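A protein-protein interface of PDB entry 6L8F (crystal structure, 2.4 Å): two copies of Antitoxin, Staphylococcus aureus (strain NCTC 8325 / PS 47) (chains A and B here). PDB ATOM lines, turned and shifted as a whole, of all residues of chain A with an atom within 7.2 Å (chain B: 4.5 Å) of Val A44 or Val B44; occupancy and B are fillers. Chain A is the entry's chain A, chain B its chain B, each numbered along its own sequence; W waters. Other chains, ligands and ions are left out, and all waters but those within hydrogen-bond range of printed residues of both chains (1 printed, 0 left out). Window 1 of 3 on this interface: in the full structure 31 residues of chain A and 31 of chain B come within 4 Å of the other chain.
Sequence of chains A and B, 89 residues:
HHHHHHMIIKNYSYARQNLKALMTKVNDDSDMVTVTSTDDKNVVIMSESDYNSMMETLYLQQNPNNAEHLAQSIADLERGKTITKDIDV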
ATOM      1  N   MET A   7      18.454   7.613 -10.811  1.00  0.00           N
ATOM      2  CA  MET A   7      19.678   7.929 -10.084  1.00  0.00           C
ATOM      3  C   MET A   7      19.493   7.715  -8.582  1.00  0.00           C
ATOM      4  O   MET A   7      18.442   8.028  -8.020  1.00  0.00           O
ATOM      5  CB  MET A   7      20.104   9.372 -10.379  1.00  0.00           C
ATOM      6  CG  MET A   7      21.414   9.806  -9.743  1.00  0.00           C
ATOM      7  SD  MET A   7      22.853   8.870 -10.293  1.00  0.00           S
ATOM      8  CE  MET A   7      22.998   9.427 -11.992  1.00  0.00           C
ATOM      9  N   VAL A  26      22.180  -1.678 -10.020  1.00  0.00           N
ATOM     10  CA  VAL A  26      22.563  -0.867 -11.170  1.00  0.00           C
ATOM     11  C   VAL A  26      22.347  -1.648 -12.464  1.00  0.00           C
ATOM     12  O   VAL A  26      21.790  -1.124 -13.436  1.00  0.00           O
ATOM     13  CB  VAL A  26      24.020  -0.387 -11.006  1.00  0.00           C
ATOM     14  CG1 VAL A  26      24.689  -0.152 -12.335  1.00  0.00           C
ATOM     15  CG2 VAL A  26      24.067   0.890 -10.186  1.00  0.00           C
ATOM     16  N   ASN A  27      22.741  -2.924 -12.482  1.00  0.00           N
ATOM     17  CA  ASN A  27      22.622  -3.720 -13.698  1.00  0.00           C
ATOM     18  C   ASN A  27      21.200  -4.234 -13.916  1.00  0.00           C
ATOM     19  O   ASN A  27      20.728  -4.279 -15.058  1.00  0.00           O
ATOM     20  CB  ASN A  27      23.614  -4.885 -13.660  1.00  0.00           C
ATOM     21  CG  ASN A  27      24.943  -4.545 -14.318  1.00  0.00           C
ATOM     22  OD1 ASN A  27      25.068  -4.581 -15.540  1.00  0.00           O
ATOM     23  ND2 ASN A  27      25.943  -4.225 -13.507  1.00  0.00           N
ATOM     24  N   MET A  32      21.472   4.074 -11.846  1.00  0.00           N
ATOM     25  CA  MET A  32      22.807   4.597 -11.624  1.00  0.00           C
ATOM     26  C   MET A  32      22.919   5.030 -10.171  1.00  0.00           C
ATOM     27  O   MET A  32      21.915   5.282  -9.498  1.00  0.00           O
ATOM     28  CB  MET A  32      23.119   5.759 -12.571  1.00  0.00           C
ATOM     29  CG  MET A  32      23.234   5.327 -14.016  1.00  0.00           C
ATOM     30  SD  MET A  32      23.124   6.687 -15.178  1.00  0.00           S
ATOM     31  CE  MET A  32      21.388   7.125 -14.994  1.00  0.00           C
ATOM     32  N   VAL A  33      24.157   5.094  -9.685  1.00  0.00           N
ATOM     33  CA  VAL A  33      24.439   5.402  -8.288  1.00  0.00           C
ATOM     34  C   VAL A  33      25.488   6.508  -8.228  1.00  0.00           C
ATOM     35  O   VAL A  33      26.576   6.367  -8.796  1.00  0.00           O
ATOM     36  CB  VAL A  33      24.908   4.160  -7.507  1.00  0.00           C
ATOM     37  CG1 VAL A  33      25.563   4.557  -6.188  1.00  0.00           C
ATOM     38  CG2 VAL A  33      23.733   3.234  -7.242  1.00  0.00           C
ATOM     39  N   THR A  34      25.159   7.603  -7.548  1.00  0.00           N
ATOM     40  CA  THR A  34      26.123   8.643  -7.217  1.00  0.00           C
ATOM     41  C   THR A  34      26.600   8.429  -5.786  1.00  0.00           C
ATOM     42  O   THR A  34      25.783   8.240  -4.881  1.00  0.00           O
ATOM     43  CB  THR A  34      25.503  10.032  -7.366  1.00  0.00           C
ATOM     44  OG1 THR A  34      24.953  10.177  -8.682  1.00  0.00           O
ATOM     45  CG2 THR A  34      26.547  11.118  -7.138  1.00  0.00           C
ATOM     46  N   VAL A  35      27.915   8.445  -5.584  1.00  0.00           N
ATOM     47  CA  VAL A  35      28.510   8.293  -4.261  1.00  0.00           C
ATOM     48  C   VAL A  35      29.141   9.625  -3.876  1.00  0.00           C
ATOM     49  O   VAL A  35      30.123  10.054  -4.494  1.00  0.00           O
ATOM     50  CB  VAL A  35      29.540   7.159  -4.220  1.00  0.00           C
ATOM     51  CG1 VAL A  35      30.238   7.130  -2.871  1.00  0.00           C
ATOM     52  CG2 VAL A  35      28.865   5.823  -4.508  1.00  0.00           C
ATOM     53  N   ASN A  42      32.990  13.444  -5.957  1.00  0.00           N
ATOM     54  CA  ASN A  42      32.007  12.379  -6.061  1.00  0.00           C
ATOM     55  C   ASN A  42      32.259  11.521  -7.294  1.00  0.00           C
ATOM     56  O   ASN A  42      32.981  11.901  -8.221  1.00  0.00           O
ATOM     57  CB  ASN A  42      30.590  12.952  -6.124  1.00  0.00           C
ATOM     58  CG  ASN A  42      30.292  13.912  -4.994  1.00  0.00           C
ATOM     59  OD1 ASN A  42      31.002  13.948  -3.992  1.00  0.00           O
ATOM     60  ND2 ASN A  42      29.229  14.693  -5.147  1.00  0.00           N
ATOM     61  N   VAL A  43      31.663  10.328  -7.285  1.00  0.00           N
ATOM     62  CA  VAL A  43      31.726   9.414  -8.415  1.00  0.00           C
ATOM     63  C   VAL A  43      30.313   8.980  -8.783  1.00  0.00           C
ATOM     64  O   VAL A  43      29.378   9.060  -7.982  1.00  0.00           O
ATOM     65  CB  VAL A  43      32.612   8.175  -8.147  1.00  0.00           C
ATOM     66  CG1 VAL A  43      34.034   8.584  -7.855  1.00  0.00           C
ATOM     67  CG2 VAL A  43      32.055   7.339  -7.014  1.00  0.00           C
ATOM     68  N   VAL A  44      30.168   8.537 -10.027  1.00  0.00           N
ATOM     69  CA  VAL A  44      28.918   7.994 -10.547  1.00  0.00           C
ATOM     70  C   VAL A  44      29.204   6.574 -11.013  1.00  0.00           C
ATOM     71  O   VAL A  44      30.197   6.337 -11.713  1.00  0.00           O
ATOM     72  CB  VAL A  44      28.349   8.862 -11.690  1.00  0.00           C
ATOM     73  CG1 VAL A  44      27.143   8.197 -12.353  1.00  0.00           C
ATOM     74  CG2 VAL A  44      27.957  10.227 -11.162  1.00  0.00           C
ATOM     75  N   ILE A  45      28.365   5.632 -10.591  1.00  0.00           N
ATOM     76  CA  ILE A  45      28.474   4.230 -10.979  1.00  0.00           C
ATOM     77  C   ILE A  45      27.317   3.907 -11.913  1.00  0.00           C
ATOM     78  O   ILE A  45      26.163   4.246 -11.624  1.00  0.00           O
ATOM     79  CB  ILE A  45      28.457   3.295  -9.757  1.00  0.00           C
ATOM     80  CG1 ILE A  45      29.496   3.723  -8.728  1.00  0.00           C
ATOM     81  CG2 ILE A  45      28.707   1.842 -10.170  1.00  0.00           C
ATOM     82  CD1 ILE A  45      29.405   2.937  -7.441  1.00  0.00           C
ATOM     83  N   MET A  46      27.626   3.253 -13.026  1.00  0.00           N
ATOM     84  CA  MET A  46      26.617   2.798 -13.966  1.00  0.00           C
ATOM     85  C   MET A  46      27.077   1.464 -14.520  1.00  0.00           C
ATOM     86  O   MET A  46      28.234   1.079 -14.362  1.00  0.00           O
ATOM     87  CB  MET A  46      26.399   3.812 -15.093  1.00  0.00           C
ATOM     88  CG  MET A  46      27.534   3.862 -16.094  1.00  0.00           C
ATOM     89  SD  MET A  46      27.393   5.286 -17.183  1.00  0.00           S
ATOM     90  CE  MET A  46      27.422   6.577 -15.961  1.00  0.00           C
ATOM     91  N   SER A  47      26.164   0.757 -15.178  1.00  0.00           N
ATOM     92  CA  SER A  47      26.516  -0.516 -15.785  1.00  0.00           C
ATOM     93  C   SER A  47      27.468  -0.299 -16.955  1.00  0.00           C
ATOM     94  O   SER A  47      27.547   0.789 -17.530  1.00  0.00           O
ATOM     95  CB  SER A  47      25.268  -1.245 -16.271  1.00  0.00           C
ATOM     96  OG  SER A  47      24.704  -0.576 -17.381  1.00  0.00           O
ATOM     97  N   GLU A  48      28.220  -1.351 -17.286  1.00  0.00           N
ATOM     98  CA  GLU A  48      29.110  -1.287 -18.440  1.00  0.00           C
ATOM     99  C   GLU A  48      28.328  -1.098 -19.738  1.00  0.00           C
ATOM    100  O   GLU A  48      28.794  -0.391 -20.643  1.00  0.00           O
ATOM    101  CB  GLU A  48      29.975  -2.548 -18.505  1.00  0.00           C
ATOM    102  CG  GLU A  48      30.995  -2.528 -19.631  1.00  0.00           C
ATOM    103  CD  GLU A  48      32.147  -3.482 -19.415  1.00  0.00           C
ATOM    104  OE1 GLU A  48      31.920  -4.594 -18.886  1.00  0.00           O
ATOM    105  OE2 GLU A  48      33.283  -3.106 -19.775  1.00  0.00           O
ATOM    106  N   SER A  49      27.123  -1.675 -19.819  1.00  0.00           N
ATOM    107  CA  SER A  49      26.260  -1.488 -20.984  1.00  0.00           C
ATOM    108  C   SER A  49      25.858  -0.026 -21.157  1.00  0.00           C
ATOM    109  O   SER A  49      25.934   0.522 -22.263  1.00  0.00           O
ATOM    110  CB  SER A  49      25.014  -2.364 -20.856  1.00  0.00           C
ATOM    111  OG  SER A  49      25.334  -3.735 -21.003  1.00  0.00           O
ATOM    112  N   ASP A  50      25.441   0.621 -20.065  1.00  0.00           N
ATOM    113  CA  ASP A  50      25.024   2.020 -20.117  1.00  0.00           C
ATOM    114  C   ASP A  50      26.190   2.941 -20.454  1.00  0.00           C
ATOM    115  O   ASP A  50      26.022   3.907 -21.205  1.00  0.00           O
ATOM    116  CB  ASP A  50      24.400   2.430 -18.785  1.00  0.00           C
ATOM    117  CG  ASP A  50      22.988   1.919 -18.625  1.00  0.00           C
ATOM    118  OD1 ASP A  50      22.268   1.861 -19.646  1.00  0.00           O
ATOM    119  OD2 ASP A  50      22.599   1.579 -17.483  1.00  0.00           O
ATOM    120  N   TYR A  51      27.374   2.648 -19.909  1.00  0.00           N
ATOM    121  CA  TYR A  51      28.573   3.411 -20.240  1.00  0.00           C
ATOM    122  C   TYR A  51      28.933   3.284 -21.716  1.00  0.00           C
ATOM    123  O   TYR A  51      29.179   4.296 -22.387  1.00  0.00           O
ATOM    124  CB  TYR A  51      29.742   2.941 -19.376  1.00  0.00           C
ATOM    125  CG  TYR A  51      31.068   3.531 -19.792  1.00  0.00           C
ATOM    126  CD1 TYR A  51      31.328   4.873 -19.599  1.00  0.00           C
ATOM    127  CD2 TYR A  51      32.056   2.747 -20.373  1.00  0.00           C
ATOM    128  CE1 TYR A  51      32.534   5.434 -19.962  1.00  0.00           C
ATOM    129  CE2 TYR A  51      33.270   3.299 -20.746  1.00  0.00           C
ATOM    130  CZ  TYR A  51      33.501   4.647 -20.536  1.00  0.00           C
ATOM    131  OH  TYR A  51      34.702   5.224 -20.893  1.00  0.00           O
ATOM    132  N   ASN A  52      28.965   2.048 -22.233  1.00  0.00           N
ATOM    133  CA  ASN A  52      29.250   1.824 -23.650  1.00  0.00           C
ATOM    134  C   ASN A  52      28.182   2.444 -24.545  1.00  0.00           C
ATOM    135  O   ASN A  52      28.514   3.016 -25.588  1.00  0.00           O
ATOM    136  CB  ASN A  52      29.380   0.327 -23.937  1.00  0.00           C
ATOM    137  CG  ASN A  52      30.652  -0.269 -23.369  1.00  0.00           C
ATOM    138  OD1 ASN A  52      31.661   0.418 -23.234  1.00  0.00           O
ATOM    139  ND2 ASN A  52      30.609  -1.552 -23.035  1.00  0.00           N
ATOM    140  N   VAL B  33      37.051   3.420 -14.018  1.00  0.00           N
ATOM    141  CA  VAL B  33      37.287   2.095 -13.449  1.00  0.00           C
ATOM    142  C   VAL B  33      36.141   1.181 -13.851  1.00  0.00           C
ATOM    143  O   VAL B  33      34.985   1.452 -13.512  1.00  0.00           O
ATOM    144  CB  VAL B  33      37.422   2.119 -11.916  1.00  0.00           C
ATOM    145  CG1 VAL B  33      37.562   0.698 -11.384  1.00  0.00           C
ATOM    146  CG2 VAL B  33      38.609   2.962 -11.472  1.00  0.00           C
ATOM    147  N   THR B  34      36.460   0.098 -14.559  1.00  0.00           N
ATOM    148  CA  THR B  34      35.531  -1.016 -14.722  1.00  0.00           C
ATOM    149  C   THR B  34      35.754  -1.992 -13.573  1.00  0.00           C
ATOM    150  O   THR B  34      36.876  -2.468 -13.369  1.00  0.00           O
ATOM    151  CB  THR B  34      35.720  -1.723 -16.067  1.00  0.00           C
ATOM    152  OG1 THR B  34      35.151  -0.933 -17.115  1.00  0.00           O
ATOM    153  CG2 THR B  34      35.024  -3.081 -16.071  1.00  0.00           C
ATOM    154  N   VAL B  43      30.276  -3.020 -13.781  1.00  0.00           N
ATOM    155  CA  VAL B  43      29.920  -1.615 -13.659  1.00  0.00           C
ATOM    156  C   VAL B  43      31.110  -0.760 -14.066  1.00  0.00           C
ATOM    157  O   VAL B  43      32.247  -1.229 -14.142  1.00  0.00           O
ATOM    158  CB  VAL B  43      29.450  -1.239 -12.237  1.00  0.00           C
ATOM    159  CG1 VAL B  43      28.081  -1.849 -11.938  1.00  0.00           C
ATOM    160  CG2 VAL B  43      30.481  -1.657 -11.202  1.00  0.00           C
ATOM    161  N   VAL B  44      30.829   0.513 -14.345  1.00  0.00           N
ATOM    162  CA  VAL B  44      31.845   1.506 -14.682  1.00  0.00           C
ATOM    163  C   VAL B  44      31.723   2.649 -13.681  1.00  0.00           C
ATOM    164  O   VAL B  44      30.613   3.107 -13.390  1.00  0.00           O
ATOM    165  CB  VAL B  44      31.699   2.006 -16.137  1.00  0.00           C
ATOM    166  CG1 VAL B  44      32.612   3.201 -16.423  1.00  0.00           C
ATOM    167  CG2 VAL B  44      32.010   0.892 -17.122  1.00  0.00           C
ATOM    168  N   ILE B  45      32.860   3.078 -13.130  1.00  0.00           N
ATOM    169  CA  ILE B  45      32.929   4.182 -12.176  1.00  0.00           C
ATOM    170  C   ILE B  45      33.675   5.341 -12.820  1.00  0.00           C
ATOM    171  O   ILE B  45      34.817   5.183 -13.268  1.00  0.00           O
ATOM    172  CB  ILE B  45      33.628   3.760 -10.871  1.00  0.00           C
ATOM    173  CG1 ILE B  45      32.952   2.535 -10.257  1.00  0.00           C
ATOM    174  CG2 ILE B  45      33.641   4.912  -9.883  1.00  0.00           C
ATOM    175  CD1 ILE B  45      33.688   1.994  -9.049  1.00  0.00           C
ATOM    176  N   MET B  46      33.044   6.506 -12.846  1.00  0.00           N
ATOM    177  CA  MET B  46      33.648   7.717 -13.372  1.00  0.00           C
ATOM    178  C   MET B  46      33.384   8.842 -12.388  1.00  0.00           C
ATOM    179  O   MET B  46      32.562   8.706 -11.482  1.00  0.00           O
ATOM    180  CB  MET B  46      33.070   8.081 -14.739  1.00  0.00           C
ATOM    181  CG  MET B  46      31.626   8.537 -14.654  1.00  0.00           C
ATOM    182  SD  MET B  46      30.914   8.775 -16.280  1.00  0.00           S
ATOM    183  CE  MET B  46      30.988   7.105 -16.882  1.00  0.00           C
ATOM    184  N   SER B  47      34.073   9.964 -12.573  1.00  0.00           N
ATOM    185  CA  SER B  47      33.798  11.116 -11.729  1.00  0.00           C
ATOM    186  C   SER B  47      32.439  11.708 -12.086  1.00  0.00           C
ATOM    187  O   SER B  47      31.963  11.576 -13.219  1.00  0.00           O
ATOM    188  CB  SER B  47      34.900  12.170 -11.869  1.00  0.00           C
ATOM    189  OG  SER B  47      34.837  12.846 -13.113  1.00  0.00           O
ATOM    190  N   GLU B  48      31.795  12.329 -11.087  1.00  0.00           N
ATOM    191  CA  GLU B  48      30.514  12.991 -11.319  1.00  0.00           C
ATOM    192  C   GLU B  48      30.665  14.138 -12.313  1.00  0.00           C
ATOM    193  O   GLU B  48      29.769  14.375 -13.137  1.00  0.00           O
ATOM    194  CB  GLU B  48      29.926  13.498  -9.997  1.00  0.00           C
ATOM    195  CG  GLU B  48      28.638  14.312 -10.169  1.00  0.00           C
ATOM    196  CD  GLU B  48      27.969  14.713  -8.878  1.00  0.00           C
ATOM    197  OE1 GLU B  48      28.676  14.960  -7.882  1.00  0.00           O
ATOM    198  OE2 GLU B  48      26.720  14.786  -8.865  1.00  0.00           O
ATOM    199  N   TYR B  51      30.656  12.602 -15.637  1.00  0.00           N
ATOM    200  CA  TYR B  51      29.304  12.140 -15.947  1.00  0.00           C
ATOM    201  C   TYR B  51      28.406  13.293 -16.370  1.00  0.00           C
ATOM    202  O   TYR B  51      27.682  13.187 -17.363  1.00  0.00           O
ATOM    203  CB  TYR B  51      28.675  11.408 -14.761  1.00  0.00           C
ATOM    204  CG  TYR B  51      27.212  11.068 -15.009  1.00  0.00           C
ATOM    205  CD1 TYR B  51      26.860  10.059 -15.898  1.00  0.00           C
ATOM    206  CD2 TYR B  51      26.183  11.771 -14.378  1.00  0.00           C
ATOM    207  CE1 TYR B  51      25.523   9.735 -16.142  1.00  0.00           C
ATOM    208  CE2 TYR B  51      24.849  11.467 -14.621  1.00  0.00           C
ATOM    209  CZ  TYR B  51      24.525  10.445 -15.498  1.00  0.00           C
ATOM    210  OH  TYR B  51      23.204  10.142 -15.740  1.00  0.00           O
HETATM  211  O   HOH W   1      33.328  14.641  -9.659  1.00  0.00           O
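Printed residues of chain A that touch a printed residue of chain B: Met A7, Val A26, Asn A27, Met A32, Asn A42, Val A43, Val A44, Ile A45, Met A46, Glu A48 and Tyr A51. Hydrophobic or aromatic side chains of chain A that line the printed part of chain B: Met A7, Val A26, Met A32, Val A43, Val A44, Ile A45, Met A46 and Tyr A51. Among the printed residues, no Asp or Glu carboxylate lies within 4 Å of a Lys or Arg side-chain nitrogen of the other chain.
Among the printed residues, merely in contact across the chains: Met A7 with Tyr B51 (3.8 Å), Val A26 with Val B43 (3.8 Å), Asn A27 with Val B43 (3.6 Å), Asn A42 with Ser B47 (3.7 Å), Val A43 with Ile B45 (3.8 Å), Val A43 with Met B46 (3.3 Å), Val A43 with Glu B48 (3.95 Å), Val A44 with Val B44 (3.7 Å), Val A44 with Ile B45 (3.5 Å), Val A44 with Glu B48 (3.8 Å), Val A44 with Tyr B51 (3.9 Å), Ile A45 with Val B43 (3.8 Å), Ile A45 with Val B44 (3.4 Å), Ile A45 with Ile B45 (3.96 Å), Met A46 with Val B43 (3.3 Å), Met A46 with Met B46 (3.7 Å), Met A46 with Tyr B51 (3.5 Å), Glu A48 with Thr B34 (3.9 Å), Glu A48 with Val B44 (3.9 Å), Tyr A51 with Val B44 (3.7 Å) and Tyr A51 with Met B46 (3.5 Å).
Printed residues of chain B within 4 Å of Met A7: Tyr B51 (3.8 Å). Of chain B, only Val B44 (3.7 Å), Ile B45 (3.5 Å), Met B46 (2.8 Å), Glu B48 (3.8 Å) and Tyr B51 (3.9 Å) come within 4 Å of Val A44. Printed residues of chain B within 4 Å of Met A46: Val B43 (3.3 Å), Val B44 (2.7 Å), Met B46 (3.7 Å) and Tyr B51 (3.5 Å). Of chain A, only Val A44, Ile A45, Met A46, Glu A48 and Tyr A51 come within 4 Å of Val B44. The nearest residue of chain A that does not touch Val B44 is Ser A47 (4.3 Å).
O of Val B33 sits at hydrogen-bond distance from N of Ile B45 (2.7 Å). SD of Met A7 sits at hydrogen-bond distance from OG1 of Thr A34. N of Ile A45 sits at hydrogen-bond distance from O of Val A33 (2.6 Å). O of Val A43 sits at hydrogen-bond distance from N of Val A35 (2.9 Å). SD of Met A46 lies close to N of Tyr A51, at 3.8 Å. O of Glu A48 lies within hydrogen-bond range of ND2 of Asn A52, 3.2 Å away.
Val A44 touches its own counterpart, Val B44. Val A44 touches Ile B45, and with the chains exchanged Ile A45 touches Val B44. Val A44 touches Met B46, and with the chains exchanged Met A46 touches Val B44. Val A44 touches Tyr B51, and with the chains exchanged Tyr A51 touches Val B44. Of the 25 pairs that touch across the chains among the printed residues, 17 have their exchanged pair printed and touching as well.
The backbone NH (N) of Val B44 lies within hydrogen-bond range of the backbone carbonyl oxygen (O) of Met A46, at 2.7 Å. O of Met B46 lies within hydrogen-bond range of N of Val A44. The side-chain carboxylate (OE1) of Glu B48 sits at hydrogen-bond distance from the side-chain amide nitrogen (ND2) of Asn A42. The side-chain hydroxyl (OH) of Tyr B51 lies within hydrogen-bond range of the side-chain sulfur (SD) of Met A32, 3.5 Å away.
Water W1 lies within hydrogen-bond range of the backbone carbonyl oxygen of Asn A42 (3.1 Å) and the backbone NH of Glu B48 (3.1 Å).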
